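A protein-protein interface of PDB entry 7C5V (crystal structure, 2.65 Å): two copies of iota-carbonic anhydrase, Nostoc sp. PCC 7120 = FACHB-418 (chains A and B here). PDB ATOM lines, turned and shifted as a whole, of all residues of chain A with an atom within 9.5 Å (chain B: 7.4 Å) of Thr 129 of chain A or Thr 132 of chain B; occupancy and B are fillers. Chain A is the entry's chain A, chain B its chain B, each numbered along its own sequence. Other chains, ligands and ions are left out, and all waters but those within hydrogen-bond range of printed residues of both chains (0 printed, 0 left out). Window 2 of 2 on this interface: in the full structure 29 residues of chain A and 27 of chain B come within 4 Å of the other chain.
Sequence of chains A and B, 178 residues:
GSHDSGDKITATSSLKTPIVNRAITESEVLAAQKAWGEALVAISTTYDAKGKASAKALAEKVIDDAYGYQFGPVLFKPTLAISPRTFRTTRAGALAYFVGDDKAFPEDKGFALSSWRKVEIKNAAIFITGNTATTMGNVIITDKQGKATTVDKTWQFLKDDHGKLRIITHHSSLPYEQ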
ATOM      1  N   ARG A  22      10.174 -11.266  14.675  1.00  0.00           N
ATOM      2  CA  ARG A  22      10.192 -12.481  15.469  1.00  0.00           C
ATOM      3  C   ARG A  22       9.003 -13.376  15.183  1.00  0.00           C
ATOM      4  O   ARG A  22       8.985 -14.528  15.627  1.00  0.00           O
ATOM      5  CB  ARG A  22      10.214 -12.138  16.956  1.00  0.00           C
ATOM      6  CG  ARG A  22      11.209 -11.061  17.301  1.00  0.00           C
ATOM      7  CD  ARG A  22      12.452 -11.646  17.917  1.00  0.00           C
ATOM      8  NE  ARG A  22      12.171 -12.601  18.991  1.00  0.00           N
ATOM      9  CZ  ARG A  22      13.118 -13.133  19.757  1.00  0.00           C
ATOM     10  NH1 ARG A  22      14.383 -12.792  19.554  1.00  0.00           N
ATOM     11  NH2 ARG A  22      12.812 -13.993  20.722  1.00  0.00           N
ATOM     12  N   ALA A  23       8.018 -12.875  14.459  1.00  0.00           N
ATOM     13  CA  ALA A  23       6.848 -13.666  14.160  1.00  0.00           C
ATOM     14  C   ALA A  23       7.177 -14.714  13.111  1.00  0.00           C
ATOM     15  O   ALA A  23       8.110 -14.574  12.314  1.00  0.00           O
ATOM     16  CB  ALA A  23       5.699 -12.777  13.686  1.00  0.00           C
ATOM     17  N   ILE A  24       6.395 -15.779  13.135  1.00  0.00           N
ATOM     18  CA  ILE A  24       6.513 -16.897  12.214  1.00  0.00           C
ATOM     19  C   ILE A  24       5.508 -16.705  11.091  1.00  0.00           C
ATOM     20  O   ILE A  24       4.356 -16.318  11.329  1.00  0.00           O
ATOM     21  CB  ILE A  24       6.258 -18.226  12.942  1.00  0.00           C
ATOM     22  CG1 ILE A  24       7.316 -18.482  13.996  1.00  0.00           C
ATOM     23  CG2 ILE A  24       6.248 -19.371  11.965  1.00  0.00           C
ATOM     24  CD1 ILE A  24       7.202 -19.858  14.615  1.00  0.00           C
ATOM     25  N   THR A  25       5.930 -16.993   9.868  1.00  0.00           N
ATOM     26  CA  THR A  25       5.036 -16.960   8.723  1.00  0.00           C
ATOM     27  C   THR A  25       4.679 -18.379   8.287  1.00  0.00           C
ATOM     28  O   THR A  25       5.384 -19.346   8.592  1.00  0.00           O
ATOM     29  CB  THR A  25       5.670 -16.182   7.562  1.00  0.00           C
ATOM     30  OG1 THR A  25       6.625 -17.015   6.893  1.00  0.00           O
ATOM     31  CG2 THR A  25       6.372 -14.931   8.083  1.00  0.00           C
ATOM     32  N   VAL A  29       6.713 -22.004   8.560  1.00  0.00           N
ATOM     33  CA  VAL A  29       6.200 -23.244   9.142  1.00  0.00           C
ATOM     34  C   VAL A  29       6.380 -24.396   8.169  1.00  0.00           C
ATOM     35  O   VAL A  29       6.934 -25.450   8.515  1.00  0.00           O
ATOM     36  CB  VAL A  29       4.724 -23.084   9.543  1.00  0.00           C
ATOM     37  CG1 VAL A  29       4.147 -24.404   9.959  1.00  0.00           C
ATOM     38  CG2 VAL A  29       4.600 -22.114  10.680  1.00  0.00           C
ATOM     39  N   ILE A 126      -3.441 -24.983  10.936  1.00  0.00           N
ATOM     40  CA  ILE A 126      -2.228 -24.284  11.343  1.00  0.00           C
ATOM     41  C   ILE A 126      -2.661 -23.129  12.231  1.00  0.00           C
ATOM     42  O   ILE A 126      -3.658 -22.470  11.935  1.00  0.00           O
ATOM     43  CB  ILE A 126      -1.439 -23.781  10.115  1.00  0.00           C
ATOM     44  CG1 ILE A 126      -0.970 -24.959   9.258  1.00  0.00           C
ATOM     45  CG2 ILE A 126      -0.261 -22.932  10.528  1.00  0.00           C
ATOM     46  CD1 ILE A 126       0.035 -24.566   8.196  1.00  0.00           C
ATOM     47  N   PHE A 127      -1.949 -22.889  13.331  1.00  0.00           N
ATOM     48  CA  PHE A 127      -2.301 -21.793  14.239  1.00  0.00           C
ATOM     49  C   PHE A 127      -1.033 -21.020  14.590  1.00  0.00           C
ATOM     50  O   PHE A 127      -0.151 -21.544  15.275  1.00  0.00           O
ATOM     51  CB  PHE A 127      -3.008 -22.315  15.497  1.00  0.00           C
ATOM     52  CG  PHE A 127      -3.763 -21.250  16.283  1.00  0.00           C
ATOM     53  CD1 PHE A 127      -3.109 -20.134  16.800  1.00  0.00           C
ATOM     54  CD2 PHE A 127      -5.120 -21.381  16.519  1.00  0.00           C
ATOM     55  CE1 PHE A 127      -3.794 -19.166  17.519  1.00  0.00           C
ATOM     56  CE2 PHE A 127      -5.804 -20.418  17.246  1.00  0.00           C
ATOM     57  CZ  PHE A 127      -5.136 -19.311  17.745  1.00  0.00           C
ATOM     58  N   ILE A 128      -0.939 -19.773  14.131  1.00  0.00           N
ATOM     59  CA  ILE A 128       0.244 -18.952  14.362  1.00  0.00           C
ATOM     60  C   ILE A 128      -0.087 -18.006  15.501  1.00  0.00           C
ATOM     61  O   ILE A 128      -0.875 -17.071  15.345  1.00  0.00           O
ATOM     62  CB  ILE A 128       0.678 -18.194  13.103  1.00  0.00           C
ATOM     63  CG1 ILE A 128       1.279 -19.164  12.097  1.00  0.00           C
ATOM     64  CG2 ILE A 128       1.727 -17.131  13.448  1.00  0.00           C
ATOM     65  CD1 ILE A 128       1.368 -18.605  10.718  1.00  0.00           C
ATOM     66  N   THR A 129       0.501 -18.286  16.654  1.00  0.00           N
ATOM     67  CA  THR A 129       0.295 -17.551  17.890  1.00  0.00           C
ATOM     68  C   THR A 129       1.182 -16.322  17.973  1.00  0.00           C
ATOM     69  O   THR A 129       1.354 -15.770  19.061  1.00  0.00           O
ATOM     70  CB  THR A 129       0.554 -18.475  19.096  1.00  0.00           C
ATOM     71  N   GLY A 130       1.763 -15.899  16.851  1.00  0.00           N
ATOM     72  CA  GLY A 130       2.798 -14.880  16.844  1.00  0.00           C
ATOM     73  C   GLY A 130       4.207 -15.452  16.797  1.00  0.00           C
ATOM     74  O   GLY A 130       4.710 -15.844  15.737  1.00  0.00           O
ATOM     75  N   ASN A 131       4.846 -15.534  17.964  1.00  0.00           N
ATOM     76  CA  ASN A 131       6.209 -16.042  18.034  1.00  0.00           C
ATOM     77  C   ASN A 131       6.293 -17.558  17.787  1.00  0.00           C
ATOM     78  O   ASN A 131       7.335 -18.060  17.345  1.00  0.00           O
ATOM     79  CB  ASN A 131       6.791 -15.685  19.393  1.00  0.00           C
ATOM     80  CG  ASN A 131       8.246 -15.457  19.330  1.00  0.00           C
ATOM     81  OD1 ASN A 131       8.974 -16.272  18.774  1.00  0.00           O
ATOM     82  ND2 ASN A 131       8.698 -14.325  19.864  1.00  0.00           N
ATOM     83  N   THR A 132       5.238 -18.308  18.090  1.00  0.00           N
ATOM     84  CA  THR A 132       5.194 -19.745  17.851  1.00  0.00           C
ATOM     85  C   THR A 132       4.181 -20.073  16.760  1.00  0.00           C
ATOM     86  O   THR A 132       3.437 -19.215  16.284  1.00  0.00           O
ATOM     87  CB  THR A 132       4.847 -20.510  19.137  1.00  0.00           C
ATOM     88  OG1 THR A 132       3.562 -20.092  19.626  1.00  0.00           O
ATOM     89  CG2 THR A 132       5.900 -20.270  20.197  1.00  0.00           C
ATOM     90  N   ALA A 133       4.155 -21.343  16.369  1.00  0.00           N
ATOM     91  CA  ALA A 133       3.162 -21.835  15.421  1.00  0.00           C
ATOM     92  C   ALA A 133       2.930 -23.320  15.665  1.00  0.00           C
ATOM     93  O   ALA A 133       3.880 -24.087  15.855  1.00  0.00           O
ATOM     94  CB  ALA A 133       3.605 -21.588  13.977  1.00  0.00           C
ATOM     95  N   THR A 134       1.666 -23.717  15.683  1.00  0.00           N
ATOM     96  CA  THR A 134       1.294 -25.114  15.848  1.00  0.00           C
ATOM     97  C   THR A 134       0.669 -25.630  14.565  1.00  0.00           C
ATOM     98  O   THR A 134      -0.140 -24.945  13.936  1.00  0.00           O
ATOM     99  CB  THR A 134       0.315 -25.308  17.008  1.00  0.00           C
ATOM    100  OG1 THR A 134       0.844 -24.706  18.191  1.00  0.00           O
ATOM    101  CG2 THR A 134       0.087 -26.787  17.275  1.00  0.00           C
ATOM    102  N   THR A 135       1.054 -26.837  14.173  1.00  0.00           N
ATOM    103  CA  THR A 135       0.381 -27.549  13.101  1.00  0.00           C
ATOM    104  C   THR A 135      -0.190 -28.851  13.634  1.00  0.00           C
ATOM    105  O   THR A 135       0.367 -29.465  14.554  1.00  0.00           O
ATOM    106  CB  THR A 135       1.319 -27.864  11.962  1.00  0.00           C
ATOM    107  OG1 THR A 135       2.202 -28.891  12.404  1.00  0.00           O
ATOM    108  CG2 THR A 135       2.116 -26.637  11.566  1.00  0.00           C
ATOM    109  N   GLN A 156       4.824 -28.044  17.413  1.00  0.00           N
ATOM    110  CA  GLN A 156       4.885 -26.642  17.785  1.00  0.00           C
ATOM    111  C   GLN A 156       6.283 -26.155  17.458  1.00  0.00           C
ATOM    112  O   GLN A 156       7.266 -26.806  17.827  1.00  0.00           O
ATOM    113  CB  GLN A 156       4.559 -26.405  19.262  1.00  0.00           C
ATOM    114  CG  GLN A 156       3.834 -25.104  19.525  1.00  0.00           C
ATOM    115  CD  GLN A 156       3.722 -24.766  21.001  1.00  0.00           C
ATOM    116  OE1 GLN A 156       3.440 -23.618  21.361  1.00  0.00           O
ATOM    117  NE2 GLN A 156       3.929 -25.754  21.861  1.00  0.00           N
ATOM    118  N   PHE A 157       6.357 -25.035  16.740  1.00  0.00           N
ATOM    119  CA  PHE A 157       7.604 -24.428  16.316  1.00  0.00           C
ATOM    120  C   PHE A 157       7.774 -23.087  17.013  1.00  0.00           C
ATOM    121  O   PHE A 157       6.856 -22.267  17.006  1.00  0.00           O
ATOM    122  CB  PHE A 157       7.616 -24.214  14.806  1.00  0.00           C
ATOM    123  CG  PHE A 157       7.548 -25.481  14.011  1.00  0.00           C
ATOM    124  CD1 PHE A 157       8.696 -26.226  13.779  1.00  0.00           C
ATOM    125  CD2 PHE A 157       6.344 -25.914  13.478  1.00  0.00           C
ATOM    126  CE1 PHE A 157       8.647 -27.382  13.035  1.00  0.00           C
ATOM    127  CE2 PHE A 157       6.295 -27.063  12.737  1.00  0.00           C
ATOM    128  CZ  PHE A 157       7.452 -27.800  12.510  1.00  0.00           C
ATOM    129  N   LEU A 158       8.944 -22.868  17.598  1.00  0.00           N
ATOM    130  CA  LEU A 158       9.329 -21.595  18.186  1.00  0.00           C
ATOM    131  C   LEU A 158      10.409 -20.958  17.312  1.00  0.00           C
ATOM    132  O   LEU A 158      11.361 -21.637  16.914  1.00  0.00           O
ATOM    133  CB  LEU A 158       9.838 -21.816  19.612  1.00  0.00           C
ATOM    134  CG  LEU A 158      10.650 -20.736  20.323  1.00  0.00           C
ATOM    135  CD1 LEU A 158       9.792 -19.559  20.630  1.00  0.00           C
ATOM    136  CD2 LEU A 158      11.215 -21.280  21.603  1.00  0.00           C
ATOM    137  N   ILE A 168       9.320 -27.412  19.871  1.00  0.00           N
ATOM    138  CA  ILE A 168       9.180 -27.502  21.318  1.00  0.00           C
ATOM    139  C   ILE A 168       8.073 -28.448  21.723  1.00  0.00           C
ATOM    140  O   ILE A 168       7.973 -28.778  22.912  1.00  0.00           O
ATOM    141  CB  ILE A 168       8.940 -26.112  21.940  1.00  0.00           C
ATOM    142  CG1 ILE A 168       7.720 -25.443  21.301  1.00  0.00           C
ATOM    143  CG2 ILE A 168      10.206 -25.256  21.805  1.00  0.00           C
ATOM    144  CD1 ILE A 168       7.172 -24.226  22.091  1.00  0.00           C
ATOM    145  N   ARG B  22      -1.120  -9.919  29.555  1.00  0.00           N
ATOM    146  CA  ARG B  22      -1.530 -10.939  28.595  1.00  0.00           C
ATOM    147  C   ARG B  22      -0.831 -12.275  28.832  1.00  0.00           C
ATOM    148  O   ARG B  22      -1.261 -13.292  28.275  1.00  0.00           O
ATOM    149  CB  ARG B  22      -1.237 -10.464  27.166  1.00  0.00           C
ATOM    150  CG  ARG B  22      -1.721  -9.055  26.805  1.00  0.00           C
ATOM    151  CD  ARG B  22      -3.141  -9.076  26.301  1.00  0.00           C
ATOM    152  NE  ARG B  22      -3.309 -10.089  25.263  1.00  0.00           N
ATOM    153  CZ  ARG B  22      -4.340 -10.137  24.422  1.00  0.00           C
ATOM    154  NH1 ARG B  22      -5.306  -9.235  24.511  1.00  0.00           N
ATOM    155  NH2 ARG B  22      -4.421 -11.100  23.510  1.00  0.00           N
ATOM    156  N   ALA B  23       0.233 -12.302  29.634  1.00  0.00           N
ATOM    157  CA  ALA B  23       0.999 -13.520  29.832  1.00  0.00           C
ATOM    158  C   ALA B  23       0.166 -14.567  30.576  1.00  0.00           C
ATOM    159  O   ALA B  23      -0.907 -14.288  31.117  1.00  0.00           O
ATOM    160  CB  ALA B  23       2.286 -13.223  30.599  1.00  0.00           C
ATOM    161  N   ILE B  24       0.673 -15.793  30.595  1.00  0.00           N
ATOM    162  CA  ILE B  24       0.040 -16.897  31.298  1.00  0.00           C
ATOM    163  C   ILE B  24       0.970 -17.341  32.415  1.00  0.00           C
ATOM    164  O   ILE B  24       2.186 -17.448  32.222  1.00  0.00           O
ATOM    165  CB  ILE B  24      -0.280 -18.064  30.345  1.00  0.00           C
ATOM    166  CG1 ILE B  24      -1.523 -17.755  29.503  1.00  0.00           C
ATOM    167  CG2 ILE B  24      -0.478 -19.340  31.107  1.00  0.00           C
ATOM    168  CD1 ILE B  24      -1.929 -18.900  28.589  1.00  0.00           C
ATOM    169  N   VAL B  29      -2.562 -22.096  33.966  1.00  0.00           N
ATOM    170  CA  VAL B  29      -2.510 -23.340  33.198  1.00  0.00           C
ATOM    171  C   VAL B  29      -3.166 -24.461  33.979  1.00  0.00           C
ATOM    172  O   VAL B  29      -4.050 -25.167  33.471  1.00  0.00           O
ATOM    173  CB  VAL B  29      -1.061 -23.708  32.837  1.00  0.00           C
ATOM    174  CG1 VAL B  29      -1.064 -25.003  32.101  1.00  0.00           C
ATOM    175  CG2 VAL B  29      -0.428 -22.633  31.970  1.00  0.00           C
ATOM    176  N   PHE B 127       5.217 -25.690  28.751  1.00  0.00           N
ATOM    177  CA  PHE B 127       5.941 -24.655  28.009  1.00  0.00           C
ATOM    178  C   PHE B 127       5.051 -23.416  27.947  1.00  0.00           C
ATOM    179  O   PHE B 127       4.007 -23.421  27.285  1.00  0.00           O
ATOM    180  CB  PHE B 127       6.306 -25.159  26.616  1.00  0.00           C
ATOM    181  CG  PHE B 127       7.491 -24.468  25.995  1.00  0.00           C
ATOM    182  CD1 PHE B 127       7.419 -23.130  25.604  1.00  0.00           C
ATOM    183  CD2 PHE B 127       8.678 -25.162  25.774  1.00  0.00           C
ATOM    184  CE1 PHE B 127       8.511 -22.494  25.012  1.00  0.00           C
ATOM    185  CE2 PHE B 127       9.768 -24.533  25.178  1.00  0.00           C
ATOM    186  CZ  PHE B 127       9.682 -23.193  24.805  1.00  0.00           C
ATOM    187  N   ILE B 128       5.431 -22.369  28.666  1.00  0.00           N
ATOM    188  CA  ILE B 128       4.724 -21.093  28.621  1.00  0.00           C
ATOM    189  C   ILE B 128       5.474 -20.235  27.616  1.00  0.00           C
ATOM    190  O   ILE B 128       6.539 -19.695  27.918  1.00  0.00           O
ATOM    191  CB  ILE B 128       4.634 -20.432  29.998  1.00  0.00           C
ATOM    192  CG1 ILE B 128       3.677 -21.243  30.884  1.00  0.00           C
ATOM    193  CG2 ILE B 128       4.120 -19.040  29.860  1.00  0.00           C
ATOM    194  CD1 ILE B 128       3.861 -21.055  32.378  1.00  0.00           C
ATOM    195  N   THR B 129       4.924 -20.159  26.407  1.00  0.00           N
ATOM    196  CA  THR B 129       5.474 -19.374  25.298  1.00  0.00           C
ATOM    197  C   THR B 129       4.678 -18.083  25.166  1.00  0.00           C
ATOM    198  O   THR B 129       3.788 -17.965  24.319  1.00  0.00           O
ATOM    199  CB  THR B 129       5.414 -20.175  23.997  1.00  0.00           C
ATOM    200  N   GLY B 130       4.993 -17.124  26.049  1.00  0.00           N
ATOM    201  CA  GLY B 130       4.341 -15.817  26.059  1.00  0.00           C
ATOM    202  C   GLY B 130       2.885 -15.760  26.516  1.00  0.00           C
ATOM    203  O   GLY B 130       2.579 -15.923  27.705  1.00  0.00           O
ATOM    204  N   ASN B 131       1.966 -15.502  25.586  1.00  0.00           N
ATOM    205  CA  ASN B 131       0.549 -15.459  25.929  1.00  0.00           C
ATOM    206  C   ASN B 131      -0.174 -16.758  25.556  1.00  0.00           C
ATOM    207  O   ASN B 131      -1.402 -16.844  25.652  1.00  0.00           O
ATOM    208  CB  ASN B 131      -0.092 -14.192  25.317  1.00  0.00           C
ATOM    209  CG  ASN B 131      -0.614 -14.385  23.900  1.00  0.00           C
ATOM    210  OD1 ASN B 131      -1.808 -14.615  23.687  1.00  0.00           O
ATOM    211  ND2 ASN B 131       0.280 -14.253  22.916  1.00  0.00           N
ATOM    212  N   THR B 132       0.574 -17.786  25.188  1.00  0.00           N
ATOM    213  CA  THR B 132       0.054 -19.133  25.052  1.00  0.00           C
ATOM    214  C   THR B 132       0.797 -20.038  26.030  1.00  0.00           C
ATOM    215  O   THR B 132       1.861 -19.688  26.538  1.00  0.00           O
ATOM    216  CB  THR B 132       0.196 -19.634  23.600  1.00  0.00           C
ATOM    217  OG1 THR B 132       1.452 -19.204  23.058  1.00  0.00           O
ATOM    218  CG2 THR B 132      -0.898 -19.034  22.752  1.00  0.00           C
ATOM    219  N   ALA B 133       0.223 -21.195  26.331  1.00  0.00           N
ATOM    220  CA  ALA B 133       0.942 -22.186  27.124  1.00  0.00           C
ATOM    221  C   ALA B 133       0.589 -23.570  26.611  1.00  0.00           C
ATOM    222  O   ALA B 133      -0.539 -23.793  26.171  1.00  0.00           O
ATOM    223  CB  ALA B 133       0.626 -22.076  28.613  1.00  0.00           C
ATOM    224  N   THR B 134       1.570 -24.482  26.639  1.00  0.00           N
ATOM    225  CA  THR B 134       1.406 -25.870  26.204  1.00  0.00           C
ATOM    226  C   THR B 134       1.771 -26.825  27.333  1.00  0.00           C
ATOM    227  O   THR B 134       2.855 -26.718  27.922  1.00  0.00           O
ATOM    228  CB  THR B 134       2.270 -26.199  24.974  1.00  0.00           C
ATOM    229  OG1 THR B 134       2.248 -25.116  24.046  1.00  0.00           O
ATOM    230  CG2 THR B 134       1.760 -27.437  24.273  1.00  0.00           C
ATOM    231  N   GLN B 156      -2.909 -26.865  24.295  1.00  0.00           N
ATOM    232  CA  GLN B 156      -2.405 -25.503  24.158  1.00  0.00           C
ATOM    233  C   GLN B 156      -3.520 -24.522  24.493  1.00  0.00           C
ATOM    234  O   GLN B 156      -4.631 -24.618  23.960  1.00  0.00           O
ATOM    235  CB  GLN B 156      -1.836 -25.221  22.759  1.00  0.00           C
ATOM    236  CG  GLN B 156      -1.164 -23.874  22.674  1.00  0.00           C
ATOM    237  CD  GLN B 156      -0.496 -23.589  21.330  1.00  0.00           C
ATOM    238  OE1 GLN B 156       0.204 -22.578  21.182  1.00  0.00           O
ATOM    239  NE2 GLN B 156      -0.710 -24.464  20.350  1.00  0.00           N
ATOM    240  N   PHE B 157      -3.222 -23.619  25.414  1.00  0.00           N
ATOM    241  CA  PHE B 157      -4.124 -22.579  25.860  1.00  0.00           C
ATOM    242  C   PHE B 157      -3.657 -21.245  25.296  1.00  0.00           C
ATOM    243  O   PHE B 157      -2.452 -20.969  25.226  1.00  0.00           O
ATOM    244  CB  PHE B 157      -4.172 -22.519  27.394  1.00  0.00           C
ATOM    245  CG  PHE B 157      -4.668 -23.784  28.024  1.00  0.00           C
ATOM    246  CD1 PHE B 157      -6.024 -24.016  28.165  1.00  0.00           C
ATOM    247  CD2 PHE B 157      -3.776 -24.763  28.435  1.00  0.00           C
ATOM    248  CE1 PHE B 157      -6.483 -25.199  28.713  1.00  0.00           C
ATOM    249  CE2 PHE B 157      -4.221 -25.933  28.984  1.00  0.00           C
ATOM    250  CZ  PHE B 157      -5.578 -26.157  29.130  1.00  0.00           C
ATOM    251  N   LEU B 158      -4.619 -20.439  24.873  1.00  0.00           N
ATOM    252  CA  LEU B 158      -4.394 -19.062  24.480  1.00  0.00           C
ATOM    253  C   LEU B 158      -5.175 -18.185  25.448  1.00  0.00           C
ATOM    254  O   LEU B 158      -6.360 -18.431  25.697  1.00  0.00           O
ATOM    255  CB  LEU B 158      -4.834 -18.838  23.024  1.00  0.00           C
ATOM    256  CG  LEU B 158      -5.043 -17.397  22.544  1.00  0.00           C
ATOM    257  CD1 LEU B 158      -3.715 -16.714  22.314  1.00  0.00           C
ATOM    258  CD2 LEU B 158      -5.886 -17.347  21.281  1.00  0.00           C
ATOM    259  N   LYS B 159      -4.508 -17.195  26.028  1.00  0.00           N
ATOM    260  CA  LYS B 159      -5.184 -16.245  26.906  1.00  0.00           C
ATOM    261  C   LYS B 159      -5.768 -15.122  26.048  1.00  0.00           C
ATOM    262  O   LYS B 159      -5.015 -14.343  25.453  1.00  0.00           O
ATOM    263  CB  LYS B 159      -4.205 -15.709  27.943  1.00  0.00           C
ATOM    264  CG  LYS B 159      -4.770 -14.658  28.863  1.00  0.00           C
ATOM    265  CD  LYS B 159      -4.095 -14.825  30.167  1.00  0.00           C
ATOM    266  CE  LYS B 159      -4.113 -13.580  30.985  1.00  0.00           C
ATOM    267  NZ  LYS B 159      -3.288 -13.809  32.206  1.00  0.00           N
ATOM    268  N   LEU B 165      -8.257 -18.415  29.429  1.00  0.00           N
ATOM    269  CA  LEU B 165      -7.534 -19.393  28.639  1.00  0.00           C
ATOM    270  C   LEU B 165      -8.515 -20.157  27.774  1.00  0.00           C
ATOM    271  O   LEU B 165      -9.633 -20.459  28.198  1.00  0.00           O
ATOM    272  CB  LEU B 165      -6.761 -20.352  29.530  1.00  0.00           C
ATOM    273  CG  LEU B 165      -5.360 -19.897  29.909  1.00  0.00           C
ATOM    274  CD1 LEU B 165      -5.422 -18.721  30.857  1.00  0.00           C
ATOM    275  CD2 LEU B 165      -4.596 -21.052  30.539  1.00  0.00           C
ATOM    276  N   ARG B 166      -8.087 -20.465  26.555  1.00  0.00           N
ATOM    277  CA  ARG B 166      -8.935 -21.090  25.562  1.00  0.00           C
ATOM    278  C   ARG B 166      -8.147 -22.195  24.872  1.00  0.00           C
ATOM    279  O   ARG B 166      -6.989 -21.999  24.493  1.00  0.00           O
ATOM    280  CB  ARG B 166      -9.423 -20.066  24.527  1.00  0.00           C
ATOM    281  CG  ARG B 166     -10.042 -18.793  25.114  1.00  0.00           C
ATOM    282  CD  ARG B 166     -11.550 -18.739  24.888  1.00  0.00           C
ATOM    283  NE  ARG B 166     -12.213 -18.189  26.063  1.00  0.00           N
ATOM    284  CZ  ARG B 166     -13.522 -18.000  26.172  1.00  0.00           C
ATOM    285  NH1 ARG B 166     -14.327 -18.334  25.167  1.00  0.00           N
ATOM    286  NH2 ARG B 166     -14.023 -17.498  27.297  1.00  0.00           N
ATOM    287  N   ILE B 168      -6.761 -24.095  22.085  1.00  0.00           N
ATOM    288  CA  ILE B 168      -6.551 -24.009  20.646  1.00  0.00           C
ATOM    289  C   ILE B 168      -5.871 -25.244  20.078  1.00  0.00           C
ATOM    290  O   ILE B 168      -5.920 -25.445  18.855  1.00  0.00           O
ATOM    291  CB  ILE B 168      -5.763 -22.739  20.253  1.00  0.00           C
ATOM    292  CG1 ILE B 168      -4.376 -22.728  20.891  1.00  0.00           C
ATOM    293  CG2 ILE B 168      -6.525 -21.494  20.660  1.00  0.00           C
ATOM    294  CD1 ILE B 168      -3.510 -21.552  20.454  1.00  0.00           C
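Printed residues of chain A that touch a printed residue of chain B: Phe 127, Thr 129, Thr 132, Thr 134, Gln 156 and Ile 168. Hydrophobic or aromatic side chains of chain A that line the printed part of chain B: Phe 127 and Ile 168. Hydrophobic or aromatic side chains of chain B that line the printed part of chain A: Phe 127 and Ile 168. Among the printed residues, no Asp or Glu carboxylate lies within 4 Å of a Lys or Arg side-chain nitrogen of the other chain.
Phe 127 of chain A touches Ile 168 of chain B, and with the chains exchanged Ile 168 of chain A touches Phe 127 of chain B. Thr 129 of chain A touches Thr 132 of chain B, and with the chains exchanged Thr 132 of chain A touches Thr 129 of chain B. Thr 134 of chain A touches Gln 156 of chain B, and with the chains exchanged Gln 156 of chain A touches Thr 134 of chain B. Gln 156 of chain B touches its own counterpart, Gln 156 of chain A. Of the 7 pairs that touch across the chains among the printed residues, 7 have their exchanged pair printed and touching as well.
N of Phe 127 of chain A lies within hydrogen-bond range of O of Thr 134 of chain A, at 2.8 Å. The backbone NH (N) of Ile 168 of chain A sits at hydrogen-bond distance from the backbone carbonyl oxygen (O) of Gln 156 of chain A (3.0 Å). The backbone NH (N) of Phe 127 of chain B lies within hydrogen-bond range of the backbone carbonyl oxygen (O) of Thr 134 of chain B (2.7 Å). O of Thr 129 of chain B sits at hydrogen-bond distance from OG1 of Thr 132 of chain B (2.9 Å). The backbone carbonyl oxygen (O) of Gln 156 of chain B is in hydrogen-bond range of the backbone NH (N) of Ile 168 of chain B, at 2.9 Å.
Among the printed residues, pairs that only touch across the chains: Ile 168 of chain A with Phe 127 of chain B (3.5 Å), Phe 127 of chain A with Ile 168 of chain B (3.7 Å), Thr 132 of chain A with Thr 129 of chain B (3.8 Å) and Thr 129 of chain A with Thr 132 of chain B (3.97 Å).
Thr 129 of chain A touches one residue of chain B. Printed residues of chain B within 4 Å of Ile 168 of chain A: Phe 127 (3.5 Å). Of the printed residues of chain A, Phe 127 of chain B touches Ile 168. No residue of chain A comes within 4 Å of Asn 131 of chain B. Thr 132 of chain B touches just one residue of chain A: Thr 129 (3.97 Å). No residue of chain A comes within 4 Å of Ala 133 of chain B. The nearest residue of chain A that does not touch Thr 132 of chain B is Thr 132 of chain A (4.1 Å). The nearest printed residue of chain A that does not touch Thr 134 of chain B is Ile 168 of chain A (5.4 Å).
The side-chain amide nitrogen (NE2) of Gln 156 of chain B lies within hydrogen-bond range of the side-chain hydroxyl (OG1) of Thr 134 of chain A (2.7 Å). NE2 of Gln 156 of chain A sits at hydrogen-bond distance from OG1 of Thr 134 of chain B (2.8 Å). OE1 of Gln 156 of chain A sits close to OE1 of Gln 156 of chain B, at 3.4 Å.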
